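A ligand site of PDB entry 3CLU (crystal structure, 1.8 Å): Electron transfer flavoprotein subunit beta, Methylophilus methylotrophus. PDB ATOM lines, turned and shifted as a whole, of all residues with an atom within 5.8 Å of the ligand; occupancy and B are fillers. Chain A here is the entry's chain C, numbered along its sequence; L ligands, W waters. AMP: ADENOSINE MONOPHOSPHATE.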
ATOM      1  N   ALA A   6       1.022  -2.541 -12.828  1.00  0.00           N
ATOM      2  CA  ALA A   6       0.914  -3.777 -13.556  1.00  0.00           C
ATOM      3  C   ALA A   6      -0.441  -3.772 -14.238  1.00  0.00           C
ATOM      4  O   ALA A   6      -1.459  -3.525 -13.601  1.00  0.00           O
ATOM      5  CB  ALA A   6       0.986  -4.971 -12.608  1.00  0.00           C
ATOM      6  N   VAL A   7      -0.461  -4.042 -15.543  1.00  0.00           N
ATOM      7  CA  VAL A   7      -1.746  -4.065 -16.245  1.00  0.00           C
ATOM      8  C   VAL A   7      -1.921  -5.338 -17.045  1.00  0.00           C
ATOM      9  O   VAL A   7      -0.939  -5.929 -17.547  1.00  0.00           O
ATOM     10  CB  VAL A   7      -1.958  -2.830 -17.176  1.00  0.00           C
ATOM     11  CG1 VAL A   7      -1.841  -1.506 -16.423  1.00  0.00           C
ATOM     12  CG2 VAL A   7      -0.981  -2.841 -18.359  1.00  0.00           C
ATOM     13  N   LYS A   8      -3.180  -5.735 -17.227  1.00  0.00           N
ATOM     14  CA  LYS A   8      -3.513  -6.956 -17.974  1.00  0.00           C
ATOM     15  C   LYS A   8      -4.474  -6.621 -19.122  1.00  0.00           C
ATOM     16  O   LYS A   8      -5.475  -5.902 -18.943  1.00  0.00           O
ATOM     17  CB  LYS A   8      -4.154  -8.025 -17.051  1.00  0.00           C
ATOM     18  CG  LYS A   8      -4.404  -9.345 -17.804  1.00  0.00           C
ATOM     19  CD  LYS A   8      -5.159 -10.390 -16.980  1.00  0.00           C
ATOM     20  CE  LYS A   8      -5.415 -11.645 -17.804  1.00  0.00           C
ATOM     21  NZ  LYS A   8      -6.131 -12.681 -16.976  1.00  0.00           N
ATOM     22  N   ASN A  36      -7.928  -4.455 -18.945  1.00  0.00           N
ATOM     23  CA  ASN A  36      -8.723  -4.809 -17.752  1.00  0.00           C
ATOM     24  C   ASN A  36      -9.319  -3.530 -17.112  1.00  0.00           C
ATOM     25  O   ASN A  36      -8.618  -2.539 -16.900  1.00  0.00           O
ATOM     26  CB  ASN A  36      -7.859  -5.601 -16.779  1.00  0.00           C
ATOM     27  CG  ASN A  36      -8.618  -6.058 -15.564  1.00  0.00           C
ATOM     28  OD1 ASN A  36      -9.819  -6.482 -15.664  1.00  0.00           O
ATOM     29  ND2 ASN A  36      -7.968  -5.950 -14.391  1.00  0.00           N
ATOM     30  N   TRP A  38     -10.218  -2.668 -14.149  1.00  0.00           N
ATOM     31  CA  TRP A  38      -9.534  -2.292 -12.920  1.00  0.00           C
ATOM     32  C   TRP A  38      -8.253  -1.474 -13.213  1.00  0.00           C
ATOM     33  O   TRP A  38      -7.890  -0.577 -12.446  1.00  0.00           O
ATOM     34  CB  TRP A  38      -9.223  -3.527 -12.090  1.00  0.00           C
ATOM     35  CG  TRP A  38     -10.385  -3.961 -11.250  1.00  0.00           C
ATOM     36  CD1 TRP A  38     -10.650  -3.606  -9.962  1.00  0.00           C
ATOM     37  CD2 TRP A  38     -11.450  -4.800 -11.668  1.00  0.00           C
ATOM     38  NE1 TRP A  38     -11.829  -4.204  -9.535  1.00  0.00           N
ATOM     39  CE2 TRP A  38     -12.358  -4.916 -10.575  1.00  0.00           C
ATOM     40  CE3 TRP A  38     -11.728  -5.497 -12.848  1.00  0.00           C
ATOM     41  CZ2 TRP A  38     -13.512  -5.684 -10.641  1.00  0.00           C
ATOM     42  CZ3 TRP A  38     -12.894  -6.244 -12.911  1.00  0.00           C
ATOM     43  CH2 TRP A  38     -13.758  -6.330 -11.812  1.00  0.00           C
ATOM     44  N   ASP A  39      -7.594  -1.791 -14.323  1.00  0.00           N
ATOM     45  CA  ASP A  39      -6.367  -1.101 -14.683  1.00  0.00           C
ATOM     46  C   ASP A  39      -6.600   0.359 -15.072  1.00  0.00           C
ATOM     47  O   ASP A  39      -5.698   1.188 -14.887  1.00  0.00           O
ATOM     48  CB  ASP A  39      -5.594  -1.874 -15.764  1.00  0.00           C
ATOM     49  CG  ASP A  39      -5.129  -3.226 -15.260  1.00  0.00           C
ATOM     50  OD1 ASP A  39      -4.873  -3.379 -14.049  1.00  0.00           O
ATOM     51  OD2 ASP A  39      -5.011  -4.147 -16.080  1.00  0.00           O
ATOM     52  N   SER A  42      -6.439   2.025 -11.692  1.00  0.00           N
ATOM     53  CA  SER A  42      -5.085   1.999 -11.160  1.00  0.00           C
ATOM     54  C   SER A  42      -4.192   3.005 -11.891  1.00  0.00           C
ATOM     55  O   SER A  42      -3.501   3.834 -11.263  1.00  0.00           O
ATOM     56  CB  SER A  42      -4.504   0.587 -11.214  1.00  0.00           C
ATOM     57  OG  SER A  42      -4.295   0.183 -12.564  1.00  0.00           O
ATOM     58  N   VAL A  62       3.416  -2.077 -16.984  1.00  0.00           N
ATOM     59  CA  VAL A  62       4.092  -3.344 -17.266  1.00  0.00           C
ATOM     60  C   VAL A  62       3.033  -4.416 -17.427  1.00  0.00           C
ATOM     61  O   VAL A  62       2.112  -4.513 -16.606  1.00  0.00           O
ATOM     62  CB  VAL A  62       5.037  -3.764 -16.111  1.00  0.00           C
ATOM     63  CG1 VAL A  62       5.732  -5.107 -16.460  1.00  0.00           C
ATOM     64  CG2 VAL A  62       6.023  -2.666 -15.807  1.00  0.00           C
ATOM     65  N   SER A  63       3.153  -5.209 -18.491  1.00  0.00           N
ATOM     66  CA  SER A  63       2.270  -6.340 -18.716  1.00  0.00           C
ATOM     67  C   SER A  63       3.063  -7.562 -19.163  1.00  0.00           C
ATOM     68  O   SER A  63       3.983  -7.463 -19.959  1.00  0.00           O
ATOM     69  CB  SER A  63       1.205  -6.043 -19.790  1.00  0.00           C
ATOM     70  OG  SER A  63       0.109  -6.947 -19.715  1.00  0.00           O
ATOM     71  N   VAL A  64       2.640  -8.712 -18.659  1.00  0.00           N
ATOM     72  CA  VAL A  64       3.133  -9.983 -19.101  1.00  0.00           C
ATOM     73  C   VAL A  64       2.120 -10.557 -20.073  1.00  0.00           C
ATOM     74  O   VAL A  64       1.018 -10.951 -19.691  1.00  0.00           O
ATOM     75  CB  VAL A  64       3.310 -10.913 -17.918  1.00  0.00           C
ATOM     76  CG1 VAL A  64       3.845 -12.234 -18.375  1.00  0.00           C
ATOM     77  CG2 VAL A  64       4.292 -10.278 -16.886  1.00  0.00           C
ATOM     78  N   GLY A  65       2.499 -10.636 -21.333  1.00  0.00           N
ATOM     79  CA  GLY A  65       1.613 -11.248 -22.283  1.00  0.00           C
ATOM     80  C   GLY A  65       2.153 -11.159 -23.673  1.00  0.00           C
ATOM     81  O   GLY A  65       3.154 -10.497 -23.900  1.00  0.00           O
ATOM     82  N   ALA A  97      -1.703 -16.859 -11.847  1.00  0.00           N
ATOM     83  CA  ALA A  97      -1.480 -15.585 -11.124  1.00  0.00           C
ATOM     84  C   ALA A  97      -0.168 -15.548 -10.353  1.00  0.00           C
ATOM     85  O   ALA A  97       0.434 -14.469 -10.170  1.00  0.00           O
ATOM     86  CB  ALA A  97      -2.601 -15.350 -10.189  1.00  0.00           C
ATOM     87  N   VAL A 100       2.754 -15.342 -12.852  1.00  0.00           N
ATOM     88  CA  VAL A 100       2.810 -13.992 -13.430  1.00  0.00           C
ATOM     89  C   VAL A 100       3.345 -13.076 -12.325  1.00  0.00           C
ATOM     90  O   VAL A 100       4.127 -12.168 -12.595  1.00  0.00           O
ATOM     91  CB  VAL A 100       1.436 -13.523 -13.996  1.00  0.00           C
ATOM     92  CG1 VAL A 100       1.378 -11.985 -14.261  1.00  0.00           C
ATOM     93  CG2 VAL A 100       1.098 -14.289 -15.303  1.00  0.00           C
ATOM     94  N   LEU A 104       6.428 -10.620 -12.982  1.00  0.00           N
ATOM     95  CA  LEU A 104       6.316  -9.189 -12.743  1.00  0.00           C
ATOM     96  C   LEU A 104       7.371  -8.717 -11.732  1.00  0.00           C
ATOM     97  O   LEU A 104       7.969  -7.675 -11.886  1.00  0.00           O
ATOM     98  CB  LEU A 104       4.924  -8.855 -12.240  1.00  0.00           C
ATOM     99  CG  LEU A 104       3.801  -8.848 -13.286  1.00  0.00           C
ATOM    100  CD1 LEU A 104       2.462  -8.771 -12.576  1.00  0.00           C
ATOM    101  CD2 LEU A 104       3.965  -7.637 -14.186  1.00  0.00           C
ATOM    102  N   PHE A 117       1.094  -0.583  -8.188  1.00  0.00           N
ATOM    103  CA  PHE A 117      -0.358  -0.722  -8.220  1.00  0.00           C
ATOM    104  C   PHE A 117      -0.724  -1.894  -9.131  1.00  0.00           C
ATOM    105  O   PHE A 117      -0.121  -2.059 -10.194  1.00  0.00           O
ATOM    106  CB  PHE A 117      -1.015   0.520  -8.808  1.00  0.00           C
ATOM    107  CG  PHE A 117      -0.852   1.794  -7.992  1.00  0.00           C
ATOM    108  CD1 PHE A 117      -0.329   1.795  -6.707  1.00  0.00           C
ATOM    109  CD2 PHE A 117      -1.255   3.001  -8.540  1.00  0.00           C
ATOM    110  CE1 PHE A 117      -0.219   2.945  -5.996  1.00  0.00           C
ATOM    111  CE2 PHE A 117      -1.135   4.195  -7.824  1.00  0.00           C
ATOM    112  CZ  PHE A 117      -0.616   4.152  -6.551  1.00  0.00           C
ATOM    113  N   ALA A 118      -1.714  -2.653  -8.714  1.00  0.00           N
ATOM    114  CA  ALA A 118      -2.315  -3.709  -9.534  1.00  0.00           C
ATOM    115  C   ALA A 118      -3.823  -3.577  -9.377  1.00  0.00           C
ATOM    116  O   ALA A 118      -4.307  -2.956  -8.396  1.00  0.00           O
ATOM    117  CB  ALA A 118      -1.844  -5.064  -9.063  1.00  0.00           C
ATOM    118  N   GLY A 119      -4.584  -4.120 -10.302  1.00  0.00           N
ATOM    119  CA  GLY A 119      -6.042  -4.142 -10.123  1.00  0.00           C
ATOM    120  C   GLY A 119      -6.428  -5.159  -9.064  1.00  0.00           C
ATOM    121  O   GLY A 119      -5.701  -6.116  -8.819  1.00  0.00           O
ATOM    122  N   VAL A 120      -7.604  -4.997  -8.477  1.00  0.00           N
ATOM    123  CA  VAL A 120      -8.144  -5.978  -7.535  1.00  0.00           C
ATOM    124  C   VAL A 120      -8.273  -7.363  -8.169  1.00  0.00           C
ATOM    125  O   VAL A 120      -7.934  -8.360  -7.547  1.00  0.00           O
ATOM    126  CB  VAL A 120      -9.489  -5.527  -6.931  1.00  0.00           C
ATOM    127  CG1 VAL A 120     -10.243  -6.669  -6.325  1.00  0.00           C
ATOM    128  CG2 VAL A 120      -9.221  -4.440  -5.913  1.00  0.00           C
ATOM    129  N   GLN A 121      -8.809  -7.401  -9.386  1.00  0.00           N
ATOM    130  CA  GLN A 121      -8.934  -8.616 -10.104  1.00  0.00           C
ATOM    131  C   GLN A 121      -9.015  -8.350 -11.604  1.00  0.00           C
ATOM    132  O   GLN A 121      -9.101  -7.204 -12.037  1.00  0.00           O
ATOM    133  CB  GLN A 121     -10.163  -9.362  -9.653  1.00  0.00           C
ATOM    134  CG  GLN A 121     -11.441  -8.703 -10.012  1.00  0.00           C
ATOM    135  CD  GLN A 121     -12.643  -9.538  -9.610  1.00  0.00           C
ATOM    136  OE1 GLN A 121     -13.608  -9.651 -10.367  1.00  0.00           O
ATOM    137  NE2 GLN A 121     -12.565 -10.182  -8.458  1.00  0.00           N
ATOM    138  N   SER A 122      -8.958  -9.432 -12.383  1.00  0.00           N
ATOM    139  CA  SER A 122      -9.109  -9.382 -13.821  1.00  0.00           C
ATOM    140  C   SER A 122     -10.556  -9.733 -14.171  1.00  0.00           C
ATOM    141  O   SER A 122     -11.173 -10.592 -13.532  1.00  0.00           O
ATOM    142  CB  SER A 122      -8.160 -10.356 -14.556  1.00  0.00           C
ATOM    143  OG  SER A 122      -8.250 -11.676 -14.043  1.00  0.00           O
ATOM    144  N   GLN A 125     -10.533 -13.763 -15.712  1.00  0.00           N
ATOM    145  CA  GLN A 125     -10.385 -14.927 -14.834  1.00  0.00           C
ATOM    146  C   GLN A 125     -10.716 -14.614 -13.356  1.00  0.00           C
ATOM    147  O   GLN A 125     -10.995 -15.531 -12.562  1.00  0.00           O
ATOM    148  CB  GLN A 125      -9.004 -15.575 -15.023  1.00  0.00           C
ATOM    149  CG  GLN A 125      -8.665 -15.999 -16.475  1.00  0.00           C
ATOM    150  CD  GLN A 125      -9.862 -16.423 -17.395  1.00  0.00           C
ATOM    151  OE1 GLN A 125     -10.857 -16.987 -16.958  1.00  0.00           O
ATOM    152  NE2 GLN A 125      -9.733 -16.162 -18.677  1.00  0.00           N
ATOM    153  N   ALA A 126     -10.649 -13.344 -12.972  1.00  0.00           N
ATOM    154  CA  ALA A 126     -11.094 -12.900 -11.676  1.00  0.00           C
ATOM    155  C   ALA A 126     -10.392 -13.764 -10.582  1.00  0.00           C
ATOM    156  O   ALA A 126     -11.049 -14.355  -9.717  1.00  0.00           O
ATOM    157  CB  ALA A 126     -12.573 -12.981 -11.595  1.00  0.00           C
ATOM    158  N   TYR A 127      -9.053 -13.887 -10.690  1.00  0.00           N
ATOM    159  CA  TYR A 127      -8.264 -14.644  -9.701  1.00  0.00           C
ATOM    160  C   TYR A 127      -8.192 -13.849  -8.408  1.00  0.00           C
ATOM    161  O   TYR A 127      -8.155 -14.427  -7.304  1.00  0.00           O
ATOM    162  CB  TYR A 127      -6.828 -14.904 -10.176  1.00  0.00           C
ATOM    163  CG  TYR A 127      -6.698 -15.748 -11.429  1.00  0.00           C
ATOM    164  CD1 TYR A 127      -5.988 -15.274 -12.520  1.00  0.00           C
ATOM    165  CD2 TYR A 127      -7.222 -17.043 -11.501  1.00  0.00           C
ATOM    166  CE1 TYR A 127      -5.827 -16.008 -13.658  1.00  0.00           C
ATOM    167  CE2 TYR A 127      -7.078 -17.806 -12.637  1.00  0.00           C
ATOM    168  CZ  TYR A 127      -6.375 -17.275 -13.725  1.00  0.00           C
ATOM    169  OH  TYR A 127      -6.192 -17.963 -14.912  1.00  0.00           O
ATOM    170  N   ALA A 128      -8.155 -12.527  -8.562  1.00  0.00           N
ATOM    171  CA  ALA A 128      -7.921 -11.607  -7.419  1.00  0.00           C
ATOM    172  C   ALA A 128      -6.691 -12.084  -6.584  1.00  0.00           C
ATOM    173  O   ALA A 128      -6.765 -12.212  -5.333  1.00  0.00           O
ATOM    174  CB  ALA A 128      -9.165 -11.509  -6.565  1.00  0.00           C
ATOM    175  N   SER A 129      -5.580 -12.314  -7.290  1.00  0.00           N
ATOM    176  CA  SER A 129      -4.386 -12.995  -6.755  1.00  0.00           C
ATOM    177  C   SER A 129      -3.073 -12.404  -7.207  1.00  0.00           C
ATOM    178  O   SER A 129      -2.093 -12.450  -6.502  1.00  0.00           O
ATOM    179  CB  SER A 129      -4.356 -14.473  -7.188  1.00  0.00           C
ATOM    180  OG  SER A 129      -5.329 -15.221  -6.485  1.00  0.00           O
ATOM    181  N   THR A 130      -3.044 -11.854  -8.410  1.00  0.00           N
ATOM    182  CA  THR A 130      -1.753 -11.482  -9.012  1.00  0.00           C
ATOM    183  C   THR A 130      -1.000 -10.402  -8.281  1.00  0.00           C
ATOM    184  O   THR A 130       0.205 -10.533  -8.026  1.00  0.00           O
ATOM    185  CB  THR A 130      -1.958 -11.088 -10.477  1.00  0.00           C
ATOM    186  OG1 THR A 130      -2.619 -12.186 -11.114  1.00  0.00           O
ATOM    187  CG2 THR A 130      -0.650 -10.816 -11.173  1.00  0.00           C
ATOM    188  N   GLY A 131      -1.678  -9.308  -7.939  1.00  0.00           N
ATOM    189  CA  GLY A 131      -1.012  -8.220  -7.260  1.00  0.00           C
ATOM    190  C   GLY A 131      -0.446  -8.610  -5.915  1.00  0.00           C
ATOM    191  O   GLY A 131       0.658  -8.235  -5.534  1.00  0.00           O
HETATM  192  P   AMP L   1      -6.016 -11.135 -11.115  1.00  0.00           P
HETATM  193  O1P AMP L   1      -5.193 -11.445 -12.353  1.00  0.00           O
HETATM  194  O2P AMP L   1      -5.431 -11.593  -9.825  1.00  0.00           O
HETATM  195  O3P AMP L   1      -7.456 -11.490 -11.185  1.00  0.00           O
HETATM  196  O5' AMP L   1      -5.956  -9.507 -11.024  1.00  0.00           O
HETATM  197  C5' AMP L   1      -5.790  -8.681 -12.182  1.00  0.00           C
HETATM  198  C4' AMP L   1      -4.709  -7.643 -11.928  1.00  0.00           C
HETATM  199  O4' AMP L   1      -3.414  -8.218 -11.662  1.00  0.00           O
HETATM  200  C3' AMP L   1      -4.540  -6.691 -13.105  1.00  0.00           C
HETATM  201  O3' AMP L   1      -5.354  -5.543 -12.943  1.00  0.00           O
HETATM  202  C2' AMP L   1      -3.046  -6.378 -13.054  1.00  0.00           C
HETATM  203  O2' AMP L   1      -2.829  -5.292 -12.122  1.00  0.00           O
HETATM  204  C1' AMP L   1      -2.450  -7.669 -12.520  1.00  0.00           C
HETATM  205  N9  AMP L   1      -2.216  -8.665 -13.585  1.00  0.00           N
HETATM  206  C8  AMP L   1      -2.796  -9.862 -13.830  1.00  0.00           C
HETATM  207  N7  AMP L   1      -2.259 -10.463 -14.910  1.00  0.00           N
HETATM  208  C5  AMP L   1      -1.310  -9.651 -15.349  1.00  0.00           C
HETATM  209  C6  AMP L   1      -0.346  -9.662 -16.454  1.00  0.00           C
HETATM  210  N6  AMP L   1      -0.381 -10.735 -17.276  1.00  0.00           N
HETATM  211  N1  AMP L   1       0.511  -8.626 -16.578  1.00  0.00           N
HETATM  212  C2  AMP L   1       0.483  -7.601 -15.724  1.00  0.00           C
HETATM  213  N3  AMP L   1      -0.366  -7.508 -14.689  1.00  0.00           N
HETATM  214  C4  AMP L   1      -1.272  -8.481 -14.482  1.00  0.00           C
HETATM  215  O   HOH W   1      -4.942 -12.798 -14.428  1.00  0.00           O
HETATM  216  O   HOH W   2      -2.200 -13.074 -13.758  1.00  0.00           O
HETATM  217  O   HOH W   3      -3.202  -1.945 -12.238  1.00  0.00           O
HETATM  218  O   HOH W   4      -4.534  -8.770  -8.425  1.00  0.00           O
HETATM  219  O   HOH W   5      -2.070 -13.338 -17.659  1.00  0.00           O
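The side-chain carboxylate (OD2) of Asp 39 is in hydrogen-bond range of the backbone NH (N) of Lys 8 (2.7 Å). The side-chain hydroxyl (OG) of Ser 42 sits at hydrogen-bond distance from the backbone carbonyl oxygen (O) of Asp 39 (2.9 Å). The side-chain hydroxyl (OG) of Ser 129 is in hydrogen-bond range of the backbone carbonyl oxygen (O) of Tyr 127, 3.0 Å away. The backbone NH (N) of Ala 6 sits at hydrogen-bond distance from the backbone carbonyl oxygen (O) of Phe 117 (2.9 Å). The backbone carbonyl oxygen (O) of Val 7 lies within hydrogen-bond range of the side-chain hydroxyl (OG) of Ser 63 (2.6 Å). The backbone NH of Val 7 lies within hydrogen-bond range of the backbone carbonyl oxygen of Val 62, at 2.8 Å. The backbone carbonyl oxygen of Gln 121 is in hydrogen-bond range of the side-chain amide nitrogen of Asn 36, 2.9 Å away. O of Lys 8 is in hydrogen-bond range of N of Asn 36.
Water W1 lies within hydrogen-bond range of O1P of the ligand (2.5 Å) and NZ of Lys 8 (2.8 Å). Water W2 bridges OG1 of Thr 130 (2.8 Å) and N7 of the ligand (2.9 Å). Water W4 lies within hydrogen-bond range of the backbone carbonyl oxygen (O) of Gly 119 (2.9 Å), the backbone NH (N) of Gly 131 (2.9 Å), an oxygen (O5') of the ligand (3.1 Å) and the backbone NH (N) of Thr 130 (3.4 Å). Water W3 lies within hydrogen-bond range of OG of Ser 42, O of Ala 6, OD1 of Asp 39, N of Gly 119 and O2' of the ligand.
OD1 of Asp 39 is in hydrogen-bond range of O3' of the ligand (2.5 Å). The backbone NH of Ser 129 lies within hydrogen-bond range of an oxygen (O2P) of the ligand (2.6 Å). O of Ala 6 lies within hydrogen-bond range of O2' of the ligand, 2.7 Å away. The backbone NH (N) of Thr 130 lies within hydrogen-bond range of an oxygen (O2P) of the ligand. O1P of the ligand sits at hydrogen-bond distance from OG1 of Thr 130, at 3.0 Å. An oxygen (O2') of the ligand sits at hydrogen-bond distance from the backbone NH (N) of Gly 119 (2.8 Å). N of Val 64 lies within hydrogen-bond range of N1 of the ligand (3.0 Å). N6 of the ligand lies within hydrogen-bond range of O of Val 64 (2.8 Å). The backbone NH of Ser 122 is in hydrogen-bond range of an oxygen (O3P) of the ligand (2.8 Å). The side-chain hydroxyl of Ser 122 is in hydrogen-bond range of an oxygen (O3P) of the ligand, at 3.0 Å. The backbone NH of Ala 128 is in hydrogen-bond range of an oxygen (O3P) of the ligand, at 2.9 Å. O3P of the ligand sits at hydrogen-bond distance from N of Tyr 127 (2.9 Å). ND2 of Asn 36 lies within hydrogen-bond range of O3' of the ligand.
N1 of the ligand lies close to O of Val 7, at 3.2 Å. Lys 8 touches the ligand (CD to N7, 3.6 Å). Val 62 touches the ligand (O to C2, 3.6 Å). Ser 63 touches the ligand. Val 100 touches the ligand. Leu 104 touches the ligand (CD1 to N3, 3.7 Å). Ala 118 touches the ligand. Gln 121 touches the ligand (CA to O5', 3.2 Å). Ala 126 touches the ligand (C to O3P, 3.8 Å). Of the 27 residues printed, 19 come within 4 Å of the ligand.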
